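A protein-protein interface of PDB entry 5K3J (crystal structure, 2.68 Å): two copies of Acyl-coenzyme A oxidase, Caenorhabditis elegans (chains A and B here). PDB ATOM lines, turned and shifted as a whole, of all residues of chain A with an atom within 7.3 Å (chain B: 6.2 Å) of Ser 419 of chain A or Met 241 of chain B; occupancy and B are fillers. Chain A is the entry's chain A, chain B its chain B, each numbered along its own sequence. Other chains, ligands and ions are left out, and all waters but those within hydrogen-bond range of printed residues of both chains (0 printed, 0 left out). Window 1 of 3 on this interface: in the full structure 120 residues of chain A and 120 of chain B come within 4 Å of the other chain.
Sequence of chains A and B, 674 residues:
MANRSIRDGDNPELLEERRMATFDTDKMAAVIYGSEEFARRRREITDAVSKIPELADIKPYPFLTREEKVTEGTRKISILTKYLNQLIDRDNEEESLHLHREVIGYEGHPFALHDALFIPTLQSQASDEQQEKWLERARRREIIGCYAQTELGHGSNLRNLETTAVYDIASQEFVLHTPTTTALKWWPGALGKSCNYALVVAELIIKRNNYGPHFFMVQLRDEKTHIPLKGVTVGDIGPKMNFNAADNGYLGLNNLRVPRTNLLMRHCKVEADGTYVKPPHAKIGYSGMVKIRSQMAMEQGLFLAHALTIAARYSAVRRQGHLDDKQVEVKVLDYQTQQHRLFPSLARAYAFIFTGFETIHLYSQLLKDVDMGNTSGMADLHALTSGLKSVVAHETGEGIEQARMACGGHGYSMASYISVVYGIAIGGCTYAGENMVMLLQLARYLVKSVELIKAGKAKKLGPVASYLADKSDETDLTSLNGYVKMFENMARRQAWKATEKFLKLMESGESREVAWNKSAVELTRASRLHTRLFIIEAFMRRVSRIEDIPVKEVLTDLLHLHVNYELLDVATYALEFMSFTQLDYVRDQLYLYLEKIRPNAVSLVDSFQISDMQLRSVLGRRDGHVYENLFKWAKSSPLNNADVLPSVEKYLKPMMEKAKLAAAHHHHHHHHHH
Tyr 422 of chain A touches its own counterpart, Tyr 422 of chain B. Of the 16 pairs that touch across the chains among the printed residues, 1 has its exchanged pair printed and touching as well.
The side-chain hydroxyl of Tyr 422 of chain B lies close to the side-chain carboxylate of Glu 401 of chain A, at 2.4 Å. The backbone NH (N) of Asn 242 of chain B lies close to the side-chain hydroxyl (OH) of Tyr 412 of chain A, 3.4 Å away. The backbone carbonyl oxygen (O) of Tyr 412 of chain A is in hydrogen-bond range of the backbone NH (N) of Met 241 of chain B, at 2.6 Å. N of Met 414 of chain A sits at hydrogen-bond distance from O of Pro 239 of chain B. OH of Tyr 412 of chain A is in hydrogen-bond range of O of Gly 423 of chain B, 2.6 Å away. SD of Met 241 of chain B is in hydrogen-bond range of NE of Arg 404 of chain A (3.5 Å). SD of Met 414 of chain A lies close to O of Lys 240 of chain B, at 3.5 Å.
CE of Met 241 of chain B touches OE1 of Glu 401 of chain A (3.7 Å). Ile 426 of chain B touches Glu 401 of chain A (CG1 to OE1, 3.6 Å). Ile 426 of chain B touches Arg 404 of chain A. Tyr 412 of chain A touches Lys 240 of chain B. Gly 427 of chain B touches Tyr 412 of chain A. OG of Ser 413 of chain A touches O of Pro 239 of chain B, 3.7 Å away. Met 241 of chain B touches Met 414 of chain A. Ser 419 of chain A touches Met 241 of chain B (CB to CG, 3.7 Å). Tyr 422 of chain B touches Tyr 422 of chain A (CE2 to CE2, 3.96 Å).
Hydrophobic or aromatic side chains of chain A within 4 Å of the printed part of chain B: Tyr 412, Met 414 and Tyr 422. Of the 10 printed residues of chain B, 8 touch a printed residue of chain A. Printed residues of chain B that touch a printed residue of chain A: Pro 239, Lys 240, Met 241, Asn 242, Tyr 422, Gly 423, Ile 426 and Gly 427. Among the printed residues, no Asp or Glu carboxylate lies within 4 Å of a Lys or Arg side-chain nitrogen of the other chain.
Ser 419 of chain A touches just one residue of chain B: Met 241 (3.7 Å). Printed residues of chain A within 4 Å of Lys 240 of chain B: Tyr 412 (3.5 Å) and Met 414 (3.5 Å). Printed residues of chain B within 4 Å of Tyr 412 of chain A: Lys 240, Met 241, Asn 242, Gly 423 and Gly 427. Phe 243 of chain B touches none of the printed residues of chain A. Ile 418 of chain A touches none of the printed residues of chain B.
The side-chain hydroxyl (OG) of Ser 413 of chain A lies close to the backbone NH (N) of Ala 415 of chain A (3.3 Å). The backbone carbonyl oxygen (O) of Phe 243 of chain B lies within hydrogen-bond range of the side-chain amino group (NZ) of Lys 240 of chain B (3.2 Å). SD of Met 414 of chain A lies within hydrogen-bond range of OG of Ser 419 of chain A (3.3 Å). The backbone carbonyl oxygen (O) of Ser 413 of chain A is in hydrogen-bond range of the side-chain hydroxyl (OG) of Ser 416 of chain A, at 2.9 Å. NH2 of Arg 404 of chain A lies within salt-bridge range of OE1 of Glu 401 of chain A (2.6 Å). The backbone NH (N) of Lys 240 of chain B lies within hydrogen-bond range of the side-chain amide oxygen (OD1) of Asn 244 of chain B (2.7 Å).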
ATOM      1  N   MET A 241     -12.892   2.945   9.862  1.00  0.00           N
ATOM      2  CA  MET A 241     -12.562   1.810  10.722  1.00  0.00           C
ATOM      3  C   MET A 241     -13.840   1.121  11.183  1.00  0.00           C
ATOM      4  O   MET A 241     -13.930  -0.106  11.218  1.00  0.00           O
ATOM      5  CB  MET A 241     -11.731   2.260  11.928  1.00  0.00           C
ATOM      6  CG  MET A 241     -11.480   1.147  12.933  1.00  0.00           C
ATOM      7  SD  MET A 241     -10.404   1.623  14.300  1.00  0.00           S
ATOM      8  CE  MET A 241      -9.978   0.017  14.970  1.00  0.00           C
ATOM      9  N   ASN A 242     -14.832   1.935  11.523  1.00  0.00           N
ATOM     10  CA  ASN A 242     -16.175   1.451  11.789  1.00  0.00           C
ATOM     11  C   ASN A 242     -17.169   2.594  11.657  1.00  0.00           C
ATOM     12  O   ASN A 242     -16.847   3.628  11.073  1.00  0.00           O
ATOM     13  CB  ASN A 242     -16.267   0.820  13.175  1.00  0.00           C
ATOM     14  CG  ASN A 242     -17.230  -0.344  13.211  1.00  0.00           C
ATOM     15  OD1 ASN A 242     -18.446  -0.166  13.121  1.00  0.00           O
ATOM     16  ND2 ASN A 242     -16.692  -1.549  13.335  1.00  0.00           N
ATOM     17  N   ILE A 400     -12.347  -4.518  25.841  1.00  0.00           N
ATOM     18  CA  ILE A 400     -13.184  -5.107  24.798  1.00  0.00           C
ATOM     19  C   ILE A 400     -12.397  -6.076  23.908  1.00  0.00           C
ATOM     20  O   ILE A 400     -12.920  -7.119  23.511  1.00  0.00           O
ATOM     21  CB  ILE A 400     -13.854  -4.001  23.949  1.00  0.00           C
ATOM     22  CG1 ILE A 400     -15.016  -3.387  24.737  1.00  0.00           C
ATOM     23  CG2 ILE A 400     -14.363  -4.542  22.614  1.00  0.00           C
ATOM     24  CD1 ILE A 400     -15.586  -2.132  24.125  1.00  0.00           C
ATOM     25  N   GLU A 401     -11.143  -5.747  23.608  1.00  0.00           N
ATOM     26  CA  GLU A 401     -10.273  -6.678  22.889  1.00  0.00           C
ATOM     27  C   GLU A 401     -10.059  -7.958  23.694  1.00  0.00           C
ATOM     28  O   GLU A 401     -10.077  -9.060  23.138  1.00  0.00           O
ATOM     29  CB  GLU A 401      -8.920  -6.039  22.571  1.00  0.00           C
ATOM     30  CG  GLU A 401      -8.884  -5.254  21.270  1.00  0.00           C
ATOM     31  CD  GLU A 401      -9.293  -6.093  20.068  1.00  0.00           C
ATOM     32  OE1 GLU A 401      -8.421  -6.400  19.222  1.00  0.00           O
ATOM     33  OE2 GLU A 401     -10.490  -6.444  19.969  1.00  0.00           O
ATOM     34  N   ARG A 404     -12.946 -10.165  23.320  1.00  0.00           N
ATOM     35  CA  ARG A 404     -12.983 -10.854  22.036  1.00  0.00           C
ATOM     36  C   ARG A 404     -12.051 -12.054  22.002  1.00  0.00           C
ATOM     37  O   ARG A 404     -12.471 -13.166  21.688  1.00  0.00           O
ATOM     38  CB  ARG A 404     -12.622  -9.889  20.901  1.00  0.00           C
ATOM     39  CG  ARG A 404     -12.497 -10.565  19.544  1.00  0.00           C
ATOM     40  CD  ARG A 404     -11.999  -9.607  18.471  1.00  0.00           C
ATOM     41  NE  ARG A 404     -10.710  -9.009  18.816  1.00  0.00           N
ATOM     42  CZ  ARG A 404      -9.532  -9.576  18.573  1.00  0.00           C
ATOM     43  NH1 ARG A 404      -9.471 -10.762  17.979  1.00  0.00           N
ATOM     44  NH2 ARG A 404      -8.409  -8.960  18.921  1.00  0.00           N
ATOM     45  N   GLY A 411     -13.875 -15.581  18.365  1.00  0.00           N
ATOM     46  CA  GLY A 411     -13.991 -14.172  18.698  1.00  0.00           C
ATOM     47  C   GLY A 411     -13.648 -13.283  17.515  1.00  0.00           C
ATOM     48  O   GLY A 411     -14.146 -12.161  17.398  1.00  0.00           O
ATOM     49  N   TYR A 412     -12.798 -13.798  16.632  1.00  0.00           N
ATOM     50  CA  TYR A 412     -12.346 -13.071  15.455  1.00  0.00           C
ATOM     51  C   TYR A 412     -13.442 -13.015  14.393  1.00  0.00           C
ATOM     52  O   TYR A 412     -13.437 -12.148  13.516  1.00  0.00           O
ATOM     53  CB  TYR A 412     -11.088 -13.730  14.899  1.00  0.00           C
ATOM     54  CG  TYR A 412     -10.306 -12.863  13.947  1.00  0.00           C
ATOM     55  CD1 TYR A 412      -9.435 -11.891  14.421  1.00  0.00           C
ATOM     56  CD2 TYR A 412     -10.425 -13.023  12.573  1.00  0.00           C
ATOM     57  CE1 TYR A 412      -8.713 -11.095  13.553  1.00  0.00           C
ATOM     58  CE2 TYR A 412      -9.710 -12.234  11.698  1.00  0.00           C
ATOM     59  CZ  TYR A 412      -8.853 -11.271  12.190  1.00  0.00           C
ATOM     60  OH  TYR A 412      -8.133 -10.478  11.323  1.00  0.00           O
ATOM     61  N   SER A 413     -14.383 -13.949  14.480  1.00  0.00           N
ATOM     62  CA  SER A 413     -15.515 -13.979  13.566  1.00  0.00           C
ATOM     63  C   SER A 413     -16.493 -12.861  13.895  1.00  0.00           C
ATOM     64  O   SER A 413     -16.583 -12.416  15.040  1.00  0.00           O
ATOM     65  CB  SER A 413     -16.225 -15.331  13.626  1.00  0.00           C
ATOM     66  OG  SER A 413     -17.345 -15.361  12.752  1.00  0.00           O
ATOM     67  N   MET A 414     -17.230 -12.411  12.886  1.00  0.00           N
ATOM     68  CA  MET A 414     -18.242 -11.378  13.079  1.00  0.00           C
ATOM     69  C   MET A 414     -19.447 -11.924  13.834  1.00  0.00           C
ATOM     70  O   MET A 414     -20.344 -11.175  14.217  1.00  0.00           O
ATOM     71  CB  MET A 414     -18.683 -10.805  11.732  1.00  0.00           C
ATOM     72  CG  MET A 414     -17.576 -10.096  10.987  1.00  0.00           C
ATOM     73  SD  MET A 414     -16.905  -8.726  11.940  1.00  0.00           S
ATOM     74  CE  MET A 414     -18.115  -7.466  11.569  1.00  0.00           C
ATOM     75  N   ALA A 415     -19.459 -13.238  14.036  1.00  0.00           N
ATOM     76  CA  ALA A 415     -20.530 -13.907  14.765  1.00  0.00           C
ATOM     77  C   ALA A 415     -20.409 -13.639  16.261  1.00  0.00           C
ATOM     78  O   ALA A 415     -21.326 -13.930  17.033  1.00  0.00           O
ATOM     79  CB  ALA A 415     -20.507 -15.395  14.484  1.00  0.00           C
ATOM     80  N   SER A 416     -19.265 -13.088  16.657  1.00  0.00           N
ATOM     81  CA  SER A 416     -19.022 -12.670  18.033  1.00  0.00           C
ATOM     82  C   SER A 416     -19.453 -11.216  18.228  1.00  0.00           C
ATOM     83  O   SER A 416     -19.923 -10.838  19.303  1.00  0.00           O
ATOM     84  CB  SER A 416     -17.545 -12.830  18.384  1.00  0.00           C
ATOM     85  OG  SER A 416     -16.781 -11.773  17.831  1.00  0.00           O
ATOM     86  N   TYR A 417     -19.261 -10.415  17.176  1.00  0.00           N
ATOM     87  CA  TYR A 417     -19.689  -9.010  17.092  1.00  0.00           C
ATOM     88  C   TYR A 417     -18.855  -8.066  17.966  1.00  0.00           C
ATOM     89  O   TYR A 417     -19.059  -6.850  17.950  1.00  0.00           O
ATOM     90  CB  TYR A 417     -21.176  -8.881  17.450  1.00  0.00           C
ATOM     91  CG  TYR A 417     -21.823  -7.603  16.961  1.00  0.00           C
ATOM     92  CD1 TYR A 417     -22.161  -7.443  15.621  1.00  0.00           C
ATOM     93  CD2 TYR A 417     -22.103  -6.559  17.837  1.00  0.00           C
ATOM     94  CE1 TYR A 417     -22.748  -6.280  15.169  1.00  0.00           C
ATOM     95  CE2 TYR A 417     -22.690  -5.393  17.388  1.00  0.00           C
ATOM     96  CZ  TYR A 417     -23.011  -5.261  16.055  1.00  0.00           C
ATOM     97  OH  TYR A 417     -23.596  -4.102  15.604  1.00  0.00           O
ATOM     98  N   ILE A 418     -17.897  -8.622  18.699  1.00  0.00           N
ATOM     99  CA  ILE A 418     -17.078  -7.844  19.623  1.00  0.00           C
ATOM    100  C   ILE A 418     -16.110  -6.927  18.870  1.00  0.00           C
ATOM    101  O   ILE A 418     -15.714  -5.874  19.372  1.00  0.00           O
ATOM    102  CB  ILE A 418     -16.310  -8.775  20.577  1.00  0.00           C
ATOM    103  CG1 ILE A 418     -17.289  -9.734  21.263  1.00  0.00           C
ATOM    104  CG2 ILE A 418     -15.540  -7.969  21.609  1.00  0.00           C
ATOM    105  CD1 ILE A 418     -16.632 -10.779  22.116  1.00  0.00           C
ATOM    106  N   SER A 419     -15.753  -7.320  17.651  1.00  0.00           N
ATOM    107  CA  SER A 419     -14.893  -6.495  16.808  1.00  0.00           C
ATOM    108  C   SER A 419     -15.617  -5.216  16.398  1.00  0.00           C
ATOM    109  O   SER A 419     -15.024  -4.136  16.381  1.00  0.00           O
ATOM    110  CB  SER A 419     -14.441  -7.268  15.570  1.00  0.00           C
ATOM    111  OG  SER A 419     -15.534  -7.573  14.726  1.00  0.00           O
ATOM    112  N   VAL A 420     -16.900  -5.345  16.069  1.00  0.00           N
ATOM    113  CA  VAL A 420     -17.749  -4.191  15.775  1.00  0.00           C
ATOM    114  C   VAL A 420     -17.782  -3.232  16.957  1.00  0.00           C
ATOM    115  O   VAL A 420     -17.469  -2.045  16.816  1.00  0.00           O
ATOM    116  CB  VAL A 420     -19.193  -4.602  15.447  1.00  0.00           C
ATOM    117  CG1 VAL A 420     -20.110  -3.372  15.429  1.00  0.00           C
ATOM    118  CG2 VAL A 420     -19.254  -5.363  14.132  1.00  0.00           C
ATOM    119  N   VAL A 421     -18.178  -3.765  18.109  1.00  0.00           N
ATOM    120  CA  VAL A 421     -18.220  -3.027  19.360  1.00  0.00           C
ATOM    121  C   VAL A 421     -16.886  -2.373  19.663  1.00  0.00           C
ATOM    122  O   VAL A 421     -16.835  -1.254  20.181  1.00  0.00           O
ATOM    123  CB  VAL A 421     -18.619  -3.952  20.530  1.00  0.00           C
ATOM    124  CG1 VAL A 421     -18.613  -3.188  21.849  1.00  0.00           C
ATOM    125  CG2 VAL A 421     -19.981  -4.565  20.270  1.00  0.00           C
ATOM    126  N   TYR A 422     -15.803  -3.062  19.331  1.00  0.00           N
ATOM    127  CA  TYR A 422     -14.495  -2.471  19.535  1.00  0.00           C
ATOM    128  C   TYR A 422     -14.317  -1.293  18.590  1.00  0.00           C
ATOM    129  O   TYR A 422     -13.995  -0.187  19.025  1.00  0.00           O
ATOM    130  CB  TYR A 422     -13.369  -3.468  19.308  1.00  0.00           C
ATOM    131  CG  TYR A 422     -12.022  -2.809  19.435  1.00  0.00           C
ATOM    132  CD1 TYR A 422     -11.529  -2.451  20.681  1.00  0.00           C
ATOM    133  CD2 TYR A 422     -11.272  -2.492  18.313  1.00  0.00           C
ATOM    134  CE1 TYR A 422     -10.314  -1.816  20.812  1.00  0.00           C
ATOM    135  CE2 TYR A 422     -10.052  -1.857  18.432  1.00  0.00           C
ATOM    136  CZ  TYR A 422      -9.579  -1.521  19.688  1.00  0.00           C
ATOM    137  OH  TYR A 422      -8.367  -0.888  19.838  1.00  0.00           O
ATOM    138  N   GLY A 423     -14.542  -1.528  17.297  1.00  0.00           N
ATOM    139  CA  GLY A 423     -14.389  -0.490  16.286  1.00  0.00           C
ATOM    140  C   GLY A 423     -15.198   0.759  16.578  1.00  0.00           C
ATOM    141  O   GLY A 423     -14.722   1.877  16.398  1.00  0.00           O
ATOM    142  N   ILE A 424     -16.428   0.564  17.039  1.00  0.00           N
ATOM    143  CA  ILE A 424     -17.323   1.671  17.362  1.00  0.00           C
ATOM    144  C   ILE A 424     -16.816   2.504  18.545  1.00  0.00           C
ATOM    145  O   ILE A 424     -16.583   3.709  18.415  1.00  0.00           O
ATOM    146  CB  ILE A 424     -18.748   1.160  17.675  1.00  0.00           C
ATOM    147  CG1 ILE A 424     -19.456   0.722  16.391  1.00  0.00           C
ATOM    148  CG2 ILE A 424     -19.563   2.229  18.373  1.00  0.00           C
ATOM    149  CD1 ILE A 424     -19.608   1.833  15.374  1.00  0.00           C
ATOM    150  N   ALA A 425     -16.631   1.855  19.689  1.00  0.00           N
ATOM    151  CA  ALA A 425     -16.305   2.553  20.928  1.00  0.00           C
ATOM    152  C   ALA A 425     -14.911   3.177  20.921  1.00  0.00           C
ATOM    153  O   ALA A 425     -14.718   4.265  21.462  1.00  0.00           O
ATOM    154  CB  ALA A 425     -16.439   1.603  22.101  1.00  0.00           C
ATOM    155  N   ILE A 426     -13.951   2.488  20.308  1.00  0.00           N
ATOM    156  CA  ILE A 426     -12.557   2.931  20.317  1.00  0.00           C
ATOM    157  C   ILE A 426     -12.409   4.304  19.668  1.00  0.00           C
ATOM    158  O   ILE A 426     -11.443   5.021  19.925  1.00  0.00           O
ATOM    159  CB  ILE A 426     -11.625   1.926  19.597  1.00  0.00           C
ATOM    160  CG1 ILE A 426     -10.159   2.170  19.977  1.00  0.00           C
ATOM    161  CG2 ILE A 426     -11.821   1.977  18.082  1.00  0.00           C
ATOM    162  CD1 ILE A 426      -9.898   2.124  21.455  1.00  0.00           C
ATOM    163  N   PRO B 239     -18.069 -13.592   7.401  1.00  0.00           N
ATOM    164  CA  PRO B 239     -17.170 -12.449   7.587  1.00  0.00           C
ATOM    165  C   PRO B 239     -16.396 -12.520   8.902  1.00  0.00           C
ATOM    166  O   PRO B 239     -16.852 -13.147   9.861  1.00  0.00           O
ATOM    167  CB  PRO B 239     -18.127 -11.248   7.574  1.00  0.00           C
ATOM    168  CG  PRO B 239     -19.305 -11.721   6.797  1.00  0.00           C
ATOM    169  CD  PRO B 239     -19.461 -13.161   7.186  1.00  0.00           C
ATOM    170  N   LYS B 240     -15.226 -11.893   8.933  1.00  0.00           N
ATOM    171  CA  LYS B 240     -14.393 -11.884  10.127  1.00  0.00           C
ATOM    172  C   LYS B 240     -14.007 -10.452  10.493  1.00  0.00           C
ATOM    173  O   LYS B 240     -14.331  -9.506   9.767  1.00  0.00           O
ATOM    174  CB  LYS B 240     -13.142 -12.741   9.910  1.00  0.00           C
ATOM    175  CG  LYS B 240     -13.445 -14.202   9.598  1.00  0.00           C
ATOM    176  CD  LYS B 240     -12.414 -14.812   8.655  1.00  0.00           C
ATOM    177  CE  LYS B 240     -12.422 -14.113   7.305  1.00  0.00           C
ATOM    178  NZ  LYS B 240     -12.071 -15.025   6.178  1.00  0.00           N
ATOM    179  N   MET B 241     -13.333 -10.306  11.632  1.00  0.00           N
ATOM    180  CA  MET B 241     -12.784  -9.028  12.073  1.00  0.00           C
ATOM    181  C   MET B 241     -11.961  -8.400  10.953  1.00  0.00           C
ATOM    182  O   MET B 241     -12.092  -7.212  10.659  1.00  0.00           O
ATOM    183  CB  MET B 241     -11.933  -9.226  13.330  1.00  0.00           C
ATOM    184  CG  MET B 241     -11.285  -7.962  13.864  1.00  0.00           C
ATOM    185  SD  MET B 241     -10.419  -8.254  15.419  1.00  0.00           S
ATOM    186  CE  MET B 241      -9.939  -6.590  15.872  1.00  0.00           C
ATOM    187  N   ASN B 242     -11.114  -9.219  10.335  1.00  0.00           N
ATOM    188  CA  ASN B 242     -10.414  -8.848   9.112  1.00  0.00           C
ATOM    189  C   ASN B 242     -10.090 -10.096   8.303  1.00  0.00           C
ATOM    190  O   ASN B 242     -10.743 -11.127   8.471  1.00  0.00           O
ATOM    191  CB  ASN B 242      -9.136  -8.067   9.415  1.00  0.00           C
ATOM    192  CG  ASN B 242      -8.898  -6.952   8.423  1.00  0.00           C
ATOM    193  OD1 ASN B 242      -8.561  -7.198   7.266  1.00  0.00           O
ATOM    194  ND2 ASN B 242      -9.090  -5.716   8.866  1.00  0.00           N
ATOM    195  N   PHE B 243      -9.084  -9.993   7.433  1.00  0.00           N
ATOM    196  CA  PHE B 243      -8.628 -11.110   6.606  1.00  0.00           C
ATOM    197  C   PHE B 243      -9.774 -11.622   5.738  1.00  0.00           C
ATOM    198  O   PHE B 243      -9.889 -12.820   5.485  1.00  0.00           O
ATOM    199  CB  PHE B 243      -8.059 -12.228   7.489  1.00  0.00           C
ATOM    200  CG  PHE B 243      -7.098 -13.141   6.781  1.00  0.00           C
ATOM    201  CD1 PHE B 243      -6.013 -12.625   6.092  1.00  0.00           C
ATOM    202  CD2 PHE B 243      -7.262 -14.514   6.834  1.00  0.00           C
ATOM    203  CE1 PHE B 243      -5.124 -13.461   5.454  1.00  0.00           C
ATOM    204  CE2 PHE B 243      -6.374 -15.357   6.199  1.00  0.00           C
ATOM    205  CZ  PHE B 243      -5.306 -14.832   5.506  1.00  0.00           C
ATOM    206  N   ASN B 244     -10.615 -10.698   5.277  1.00  0.00           N
ATOM    207  CA  ASN B 244     -11.876 -11.046   4.624  1.00  0.00           C
ATOM    208  C   ASN B 244     -11.773 -11.329   3.129  1.00  0.00           C
ATOM    209  O   ASN B 244     -12.743 -11.766   2.504  1.00  0.00           O
ATOM    210  CB  ASN B 244     -12.896  -9.933   4.851  1.00  0.00           C
ATOM    211  CG  ASN B 244     -13.389  -9.885   6.276  1.00  0.00           C
ATOM    212  OD1 ASN B 244     -14.074 -10.796   6.733  1.00  0.00           O
ATOM    213  ND2 ASN B 244     -13.049  -8.818   6.989  1.00  0.00           N
ATOM    214  N   TYR B 422      -4.029  -3.358  11.779  1.00  0.00           N
ATOM    215  CA  TYR B 422      -4.323  -3.824  13.122  1.00  0.00           C
ATOM    216  C   TYR B 422      -5.135  -5.110  13.065  1.00  0.00           C
ATOM    217  O   TYR B 422      -4.729  -6.128  13.625  1.00  0.00           O
ATOM    218  CB  TYR B 422      -5.083  -2.769  13.925  1.00  0.00           C
ATOM    219  CG  TYR B 422      -5.540  -3.286  15.269  1.00  0.00           C
ATOM    220  CD1 TYR B 422      -4.635  -3.460  16.306  1.00  0.00           C
ATOM    221  CD2 TYR B 422      -6.868  -3.623  15.493  1.00  0.00           C
ATOM    222  CE1 TYR B 422      -5.035  -3.944  17.527  1.00  0.00           C
ATOM    223  CE2 TYR B 422      -7.282  -4.110  16.717  1.00  0.00           C
ATOM    224  CZ  TYR B 422      -6.355  -4.268  17.730  1.00  0.00           C
ATOM    225  OH  TYR B 422      -6.741  -4.750  18.956  1.00  0.00           O
ATOM    226  N   GLY B 423      -6.278  -5.056  12.383  1.00  0.00           N
ATOM    227  CA  GLY B 423      -7.190  -6.185  12.295  1.00  0.00           C
ATOM    228  C   GLY B 423      -6.527  -7.465  11.821  1.00  0.00           C
ATOM    229  O   GLY B 423      -6.792  -8.545  12.345  1.00  0.00           O
ATOM    230  N   ILE B 426      -3.485  -8.341  14.721  1.00  0.00           N
ATOM    231  CA  ILE B 426      -3.999  -8.687  16.044  1.00  0.00           C
ATOM    232  C   ILE B 426      -4.501 -10.129  16.125  1.00  0.00           C
ATOM    233  O   ILE B 426      -4.587 -10.700  17.210  1.00  0.00           O
ATOM    234  CB  ILE B 426      -5.143  -7.727  16.470  1.00  0.00           C
ATOM    235  CG1 ILE B 426      -5.386  -7.805  17.986  1.00  0.00           C
ATOM    236  CG2 ILE B 426      -6.416  -8.018  15.675  1.00  0.00           C
ATOM    237  CD1 ILE B 426      -4.208  -7.329  18.830  1.00  0.00           C
ATOM    238  N   GLY B 427      -4.813 -10.716  14.975  1.00  0.00           N
ATOM    239  CA  GLY B 427      -5.205 -12.110  14.920  1.00  0.00           C
ATOM    240  C   GLY B 427      -4.080 -13.001  15.414  1.00  0.00           C
ATOM    241  O   GLY B 427      -4.315 -14.123  15.864  1.00  0.00           O
